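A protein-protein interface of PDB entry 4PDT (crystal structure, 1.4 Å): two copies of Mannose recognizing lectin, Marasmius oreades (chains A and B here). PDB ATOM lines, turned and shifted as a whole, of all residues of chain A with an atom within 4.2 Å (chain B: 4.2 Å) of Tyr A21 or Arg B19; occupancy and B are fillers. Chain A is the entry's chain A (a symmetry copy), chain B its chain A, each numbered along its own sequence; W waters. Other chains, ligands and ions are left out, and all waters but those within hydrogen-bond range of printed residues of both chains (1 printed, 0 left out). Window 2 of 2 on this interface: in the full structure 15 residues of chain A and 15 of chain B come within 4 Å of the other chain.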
ATOM      1  N   TYR A   3     -25.774  -7.537   6.346  1.00  0.00           N
ATOM      2  CA  TYR A   3     -25.925  -8.290   5.132  1.00  0.00           C
ATOM      3  C   TYR A   3     -27.368  -8.650   4.880  1.00  0.00           C
ATOM      4  O   TYR A   3     -28.127  -8.970   5.800  1.00  0.00           O
ATOM      5  CB  TYR A   3     -25.064  -9.557   5.146  1.00  0.00           C
ATOM      6  CG  TYR A   3     -23.596  -9.252   5.240  1.00  0.00           C
ATOM      7  CD1 TYR A   3     -22.984  -8.976   6.479  1.00  0.00           C
ATOM      8  CD2 TYR A   3     -22.827  -9.190   4.097  1.00  0.00           C
ATOM      9  CE1 TYR A   3     -21.632  -8.653   6.543  1.00  0.00           C
ATOM     10  CE2 TYR A   3     -21.480  -8.848   4.131  1.00  0.00           C
ATOM     11  CZ  TYR A   3     -20.888  -8.573   5.350  1.00  0.00           C
ATOM     12  OH  TYR A   3     -19.579  -8.204   5.374  1.00  0.00           O
ATOM     13  N   VAL A   4     -27.767  -8.460   3.614  1.00  0.00           N
ATOM     14  CA  VAL A   4     -29.115  -8.847   3.189  1.00  0.00           C
ATOM     15  C   VAL A   4     -29.123 -10.356   2.908  1.00  0.00           C
ATOM     16  O   VAL A   4     -28.145 -10.910   2.388  1.00  0.00           O
ATOM     17  CB  VAL A   4     -29.523  -8.015   1.944  1.00  0.00           C
ATOM     18  CG1 VAL A   4     -30.864  -8.496   1.375  1.00  0.00           C
ATOM     19  CG2 VAL A   4     -29.549  -6.537   2.307  1.00  0.00           C
ATOM     20  N   PRO A   6     -31.156 -13.079   0.914  1.00  0.00           N
ATOM     21  CA  PRO A   6     -32.227 -13.397  -0.083  1.00  0.00           C
ATOM     22  C   PRO A   6     -32.619 -14.849  -0.157  1.00  0.00           C
ATOM     23  O   PRO A   6     -33.530 -15.231  -0.875  1.00  0.00           O
ATOM     24  CB  PRO A   6     -31.573 -13.044  -1.413  1.00  0.00           C
ATOM     25  CG  PRO A   6     -30.254 -12.391  -1.122  1.00  0.00           C
ATOM     26  CD  PRO A   6     -29.861 -12.817   0.267  1.00  0.00           C
ATOM     27  N   ILE A  17     -24.878 -15.265  -4.193  1.00  0.00           N
ATOM     28  CA  ILE A  17     -24.801 -14.166  -3.244  1.00  0.00           C
ATOM     29  C   ILE A  17     -23.628 -13.248  -3.658  1.00  0.00           C
ATOM     30  O   ILE A  17     -22.515 -13.690  -3.917  1.00  0.00           O
ATOM     31  CB  ILE A  17     -24.753 -14.510  -1.742  1.00  0.00           C
ATOM     32  CG1 ILE A  17     -23.738 -15.581  -1.497  1.00  0.00           C
ATOM     33  CG2 ILE A  17     -26.159 -14.890  -1.236  1.00  0.00           C
ATOM     34  CD1 ILE A  17     -23.436 -15.877  -0.018  1.00  0.00           C
ATOM     35  N   GLY A  18     -23.950 -11.957  -3.766  1.00  0.00           N
ATOM     36  CA  GLY A  18     -22.962 -10.937  -4.079  1.00  0.00           C
ATOM     37  C   GLY A  18     -22.488 -10.172  -2.833  1.00  0.00           C
ATOM     38  O   GLY A  18     -22.891 -10.480  -1.700  1.00  0.00           O
ATOM     39  N   ARG A  19     -21.639  -9.187  -3.047  1.00  0.00           N
ATOM     40  CA  ARG A  19     -21.109  -8.382  -1.977  1.00  0.00           C
ATOM     41  C   ARG A  19     -22.230  -7.723  -1.249  1.00  0.00           C
ATOM     42  O   ARG A  19     -23.135  -7.070  -1.852  1.00  0.00           O
ATOM     43  CB  ARG A  19     -20.125  -7.361  -2.490  1.00  0.00           C
ATOM     44  CG  ARG A  19     -18.888  -7.909  -3.162  1.00  0.00           C
ATOM     45  CD  ARG A  19     -17.907  -6.839  -3.598  1.00  0.00           C
ATOM     46  NE  ARG A  19     -16.677  -7.464  -4.083  1.00  0.00           N
ATOM     47  CZ  ARG A  19     -15.730  -6.869  -4.789  1.00  0.00           C
ATOM     48  NH1 ARG A  19     -14.710  -7.562  -5.269  1.00  0.00           N
ATOM     49  NH2 ARG A  19     -15.777  -5.556  -4.984  1.00  0.00           N
ATOM     50  N   GLY A  20     -22.193  -7.831   0.075  1.00  0.00           N
ATOM     51  CA  GLY A  20     -23.234  -7.291   0.929  1.00  0.00           C
ATOM     52  C   GLY A  20     -24.439  -8.189   1.132  1.00  0.00           C
ATOM     53  O   GLY A  20     -25.419  -7.793   1.791  1.00  0.00           O
ATOM     54  N   TYR A  21     -24.317  -9.430   0.668  1.00  0.00           N
ATOM     55  CA  TYR A  21     -25.376 -10.429   0.835  1.00  0.00           C
ATOM     56  C   TYR A  21     -24.786 -11.632   1.528  1.00  0.00           C
ATOM     57  O   TYR A  21     -23.566 -11.810   1.517  1.00  0.00           O
ATOM     58  CB  TYR A  21     -26.032 -10.811  -0.523  1.00  0.00           C
ATOM     59  CG  TYR A  21     -26.671  -9.561  -1.201  1.00  0.00           C
ATOM     60  CD1 TYR A  21     -25.879  -8.604  -1.821  1.00  0.00           C
ATOM     61  CD2 TYR A  21     -28.043  -9.308  -1.092  1.00  0.00           C
ATOM     62  CE1 TYR A  21     -26.448  -7.460  -2.403  1.00  0.00           C
ATOM     63  CE2 TYR A  21     -28.604  -8.151  -1.621  1.00  0.00           C
ATOM     64  CZ  TYR A  21     -27.782  -7.245  -2.252  1.00  0.00           C
ATOM     65  OH  TYR A  21     -28.327  -6.073  -2.733  1.00  0.00           O
ATOM     66  N   ALA A  22     -25.650 -12.469   2.041  1.00  0.00           N
ATOM     67  CA  ALA A  22     -25.191 -13.596   2.895  1.00  0.00           C
ATOM     68  C   ALA A  22     -26.260 -14.649   3.049  1.00  0.00           C
ATOM     69  O   ALA A  22     -27.460 -14.361   2.950  1.00  0.00           O
ATOM     70  CB  ALA A  22     -24.730 -13.102   4.313  1.00  0.00           C
ATOM     71  N   ARG A  33     -20.956 -14.826   4.391  1.00  0.00           N
ATOM     72  CA  ARG A  33     -20.885 -13.504   3.767  1.00  0.00           C
ATOM     73  C   ARG A  33     -19.947 -13.332   2.618  1.00  0.00           C
ATOM     74  O   ARG A  33     -18.861 -13.915   2.609  1.00  0.00           O
ATOM     75  CB  ARG A  33     -20.301 -12.491   4.796  1.00  0.00           C
ATOM     76  CG  ARG A  33     -20.987 -12.470   6.124  1.00  0.00           C
ATOM     77  CD  ARG A  33     -20.180 -11.716   7.169  1.00  0.00           C
ATOM     78  NE  ARG A  33     -20.927 -11.623   8.416  1.00  0.00           N
ATOM     79  CZ  ARG A  33     -20.505 -11.036   9.527  1.00  0.00           C
ATOM     80  NH1 ARG A  33     -19.294 -10.506   9.574  1.00  0.00           N
ATOM     81  NH2 ARG A  33     -21.281 -11.067  10.620  1.00  0.00           N
ATOM     82  N   VAL A  34     -20.379 -12.519   1.626  1.00  0.00           N
ATOM     83  CA  VAL A  34     -19.481 -12.013   0.612  1.00  0.00           C
ATOM     84  C   VAL A  34     -19.374 -10.516   0.928  1.00  0.00           C
ATOM     85  O   VAL A  34     -20.382  -9.821   0.956  1.00  0.00           O
ATOM     86  CB  VAL A  34     -19.952 -12.242  -0.820  1.00  0.00           C
ATOM     87  CG1 VAL A  34     -18.975 -11.616  -1.799  1.00  0.00           C
ATOM     88  CG2 VAL A  34     -20.090 -13.739  -1.064  1.00  0.00           C
ATOM     89  N   GLY B  18     -28.413  -8.684  -6.905  1.00  0.00           N
ATOM     90  CA  GLY B  18     -28.378  -7.640  -5.894  1.00  0.00           C
ATOM     91  C   GLY B  18     -27.816  -6.315  -6.434  1.00  0.00           C
ATOM     92  O   GLY B  18     -27.503  -6.190  -7.630  1.00  0.00           O
ATOM     93  N   ARG B  19     -27.693  -5.338  -5.557  1.00  0.00           N
ATOM     94  CA  ARG B  19     -27.181  -4.041  -5.917  1.00  0.00           C
ATOM     95  C   ARG B  19     -25.806  -4.186  -6.472  1.00  0.00           C
ATOM     96  O   ARG B  19     -24.900  -4.838  -5.868  1.00  0.00           O
ATOM     97  CB  ARG B  19     -27.192  -3.097  -4.740  1.00  0.00           C
ATOM     98  CG  ARG B  19     -28.546  -2.789  -4.149  1.00  0.00           C
ATOM     99  CD  ARG B  19     -28.501  -1.786  -3.013  1.00  0.00           C
ATOM    100  NE  ARG B  19     -29.862  -1.425  -2.617  1.00  0.00           N
ATOM    101  CZ  ARG B  19     -30.207  -0.805  -1.500  1.00  0.00           C
ATOM    102  NH1 ARG B  19     -31.482  -0.626  -1.195  1.00  0.00           N
ATOM    103  NH2 ARG B  19     -29.268  -0.319  -0.697  1.00  0.00           N
ATOM    104  N   GLY B  20     -25.582  -3.552  -7.618  1.00  0.00           N
ATOM    105  CA  GLY B  20     -24.313  -3.632  -8.316  1.00  0.00           C
ATOM    106  C   GLY B  20     -24.148  -4.833  -9.229  1.00  0.00           C
ATOM    107  O   GLY B  20     -23.070  -5.032  -9.822  1.00  0.00           O
ATOM    108  N   TYR B  21     -25.245  -5.558  -9.429  1.00  0.00           N
ATOM    109  CA  TYR B  21     -25.255  -6.718 -10.326  1.00  0.00           C
ATOM    110  C   TYR B  21     -26.338  -6.509 -11.354  1.00  0.00           C
ATOM    111  O   TYR B  21     -27.250  -5.709 -11.134  1.00  0.00           O
ATOM    112  CB  TYR B  21     -25.449  -8.050  -9.546  1.00  0.00           C
ATOM    113  CG  TYR B  21     -24.297  -8.264  -8.519  1.00  0.00           C
ATOM    114  CD1 TYR B  21     -24.259  -7.545  -7.332  1.00  0.00           C
ATOM    115  CD2 TYR B  21     -23.209  -9.092  -8.822  1.00  0.00           C
ATOM    116  CE1 TYR B  21     -23.204  -7.711  -6.420  1.00  0.00           C
ATOM    117  CE2 TYR B  21     -22.138  -9.219  -7.944  1.00  0.00           C
ATOM    118  CZ  TYR B  21     -22.158  -8.507  -6.766  1.00  0.00           C
ATOM    119  OH  TYR B  21     -21.074  -8.591  -5.918  1.00  0.00           O
ATOM    120  N   VAL B  34     -29.775  -3.666 -10.792  1.00  0.00           N
ATOM    121  CA  VAL B  34     -30.230  -3.277  -9.475  1.00  0.00           C
ATOM    122  C   VAL B  34     -29.130  -2.337  -8.968  1.00  0.00           C
ATOM    123  O   VAL B  34     -27.972  -2.730  -8.894  1.00  0.00           O
ATOM    124  CB  VAL B  34     -30.448  -4.440  -8.514  1.00  0.00           C
ATOM    125  CG1 VAL B  34     -30.858  -3.920  -7.147  1.00  0.00           C
ATOM    126  CG2 VAL B  34     -31.512  -5.367  -9.089  1.00  0.00           C
ATOM    127  N   THR B  35     -29.504  -1.090  -8.710  1.00  0.00           N
ATOM    128  CA  THR B  35     -28.515  -0.047  -8.460  1.00  0.00           C
ATOM    129  C   THR B  35     -28.218   0.158  -6.989  1.00  0.00           C
ATOM    130  O   THR B  35     -29.036  -0.132  -6.129  1.00  0.00           O
ATOM    131  CB  THR B  35     -28.913   1.307  -9.113  1.00  0.00           C
ATOM    132  OG1 THR B  35     -29.923   1.952  -8.318  1.00  0.00           O
ATOM    133  CG2 THR B  35     -29.410   1.085 -10.581  1.00  0.00           C
ATOM    134  N   ASP B  36     -27.096   0.806  -6.736  1.00  0.00           N
ATOM    135  CA  ASP B  36     -26.712   1.162  -5.365  1.00  0.00           C
ATOM    136  C   ASP B  36     -27.731   2.131  -4.732  1.00  0.00           C
ATOM    137  O   ASP B  36     -27.877   2.167  -3.496  1.00  0.00           O
ATOM    138  CB  ASP B  36     -25.318   1.802  -5.332  1.00  0.00           C
ATOM    139  CG  ASP B  36     -24.199   0.825  -5.692  1.00  0.00           C
ATOM    140  OD1 ASP B  36     -24.335  -0.390  -5.422  1.00  0.00           O
ATOM    141  OD2 ASP B  36     -23.133   1.297  -6.166  1.00  0.00           O
ATOM    142  N   GLY B  38     -30.841   1.866  -5.007  1.00  0.00           N
ATOM    143  CA  GLY B  38     -32.109   1.152  -4.760  1.00  0.00           C
ATOM    144  C   GLY B  38     -33.139   1.147  -5.907  1.00  0.00           C
ATOM    145  O   GLY B  38     -34.332   0.927  -5.677  1.00  0.00           O
ATOM    146  N   ASN B  57     -36.326   1.617  -2.833  1.00  0.00           N
ATOM    147  CA  ASN B  57     -35.260   1.009  -1.938  1.00  0.00           C
ATOM    148  C   ASN B  57     -35.076  -0.465  -2.250  1.00  0.00           C
ATOM    149  O   ASN B  57     -34.972  -1.310  -1.342  1.00  0.00           O
ATOM    150  CB  ASN B  57     -35.613   1.216  -0.445  1.00  0.00           C
ATOM    151  CG  ASN B  57     -34.457   0.880   0.530  1.00  0.00           C
ATOM    152  OD1 ASN B  57     -33.256   1.084   0.233  1.00  0.00           O
ATOM    153  ND2 ASN B  57     -34.835   0.452   1.772  1.00  0.00           N
ATOM    154  N   ALA B  58     -35.124  -0.828  -3.516  1.00  0.00           N
ATOM    155  CA  ALA B  58     -34.894  -2.188  -3.953  1.00  0.00           C
ATOM    156  C   ALA B  58     -33.455  -2.634  -3.567  1.00  0.00           C
ATOM    157  O   ALA B  58     -32.478  -1.907  -3.750  1.00  0.00           O
ATOM    158  CB  ALA B  58     -35.089  -2.326  -5.469  1.00  0.00           C
ATOM    159  N   SER B  59     -33.389  -3.866  -3.050  1.00  0.00           N
ATOM    160  CA  SER B  59     -32.135  -4.498  -2.665  1.00  0.00           C
ATOM    161  C   SER B  59     -31.790  -5.609  -3.668  1.00  0.00           C
ATOM    162  O   SER B  59     -30.616  -5.806  -4.010  1.00  0.00           O
ATOM    163  CB  SER B  59     -32.238  -5.086  -1.259  1.00  0.00           C
ATOM    164  OG  SER B  59     -31.037  -5.751  -0.953  1.00  0.00           O
ATOM    165  N   PRO B  74     -34.328  -4.327   1.395  1.00  0.00           N
ATOM    166  CA  PRO B  74     -33.330  -5.087   2.208  1.00  0.00           C
ATOM    167  C   PRO B  74     -33.911  -5.934   3.306  1.00  0.00           C
ATOM    168  O   PRO B  74     -33.210  -6.805   3.847  1.00  0.00           O
ATOM    169  CB  PRO B  74     -32.466  -3.968   2.793  1.00  0.00           C
ATOM    170  CG  PRO B  74     -32.616  -2.798   1.859  1.00  0.00           C
ATOM    171  CD  PRO B  74     -34.057  -2.873   1.437  1.00  0.00           C
HETATM  172  O   HOH W   1     -23.608  -5.128  -3.581  1.00  0.00           O
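The side-chain hydroxyl (OH) of Tyr A21 sits at hydrogen-bond distance from the backbone NH (N) of Arg B19 (3.0 Å).
The side-chain hydroxyl (OH) of Tyr B21 is in hydrogen-bond range of the backbone NH (N) of Arg A19 (3.0 Å).
The side-chain hydroxyl of Tyr A21 is in hydrogen-bond range of the backbone carbonyl oxygen of Ser B59, at 2.6 Å.
OD1 of Asn B57 sits at hydrogen-bond distance from NH1 of Arg B19.
The guanidinium group (NE) of Arg B19 is in hydrogen-bond range of the backbone carbonyl oxygen (O) of Ala B58 (2.9 Å).
The backbone NH (N) of Arg B19 is in hydrogen-bond range of the backbone carbonyl oxygen (O) of Ser B59, at 3.3 Å.
The backbone NH of Val A4 lies within hydrogen-bond range of the backbone carbonyl oxygen of Gly A20.
O of Val A4 is in hydrogen-bond range of N of Ala A22 (3.0 Å).
O of Tyr A21 sits at hydrogen-bond distance from N of Val A34, 3.3 Å away.
Val A4 touches Ser B59 (CG1 to OG, 3.6 Å).
Val A4 touches Pro B74 (CG1 to O, 3.8 Å).
Gly A18 touches Tyr B21 (CA to OH, 3.5 Å).
Tyr A21 touches Gly B18 (OH to CA, 3.5 Å).
Printed residues of chain B within 4 Å of Gly A18: Tyr B21.
Of chain B, only Gly B18 (3.5 Å), Arg B19 (3.0 Å) and Ser B59 (2.6 Å) come within 4 Å of Tyr A21.
Arg B19 touches just one residue of chain A: Tyr A21 (3.0 Å).
Printed residues of chain A within 4 Å of Tyr B21: Gly A18 (3.5 Å) and Arg A19 (3.0 Å).
The nearest printed residue of chain B that does not touch Val A4 is Arg B19 (6.9 Å).
Printed residues of chain B that touch a printed residue of chain A: Gly B18, Arg B19, Tyr B21, Ser B59 and Pro B74.
Among the printed residues, 7 pairs touch across the chains.
Gly A18 touches Tyr B21, and with the chains exchanged Tyr A21 touches Gly B18.
Arg A19 touches Tyr B21, and with the chains exchanged Tyr A21 touches Arg B19.
Of the 7 pairs that touch across the chains among the printed residues, 4 have their exchanged pair printed and touching as well.
Water W1 bridges O of Arg A19 (2.6 Å) and O of Arg B19 (2.6 Å).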
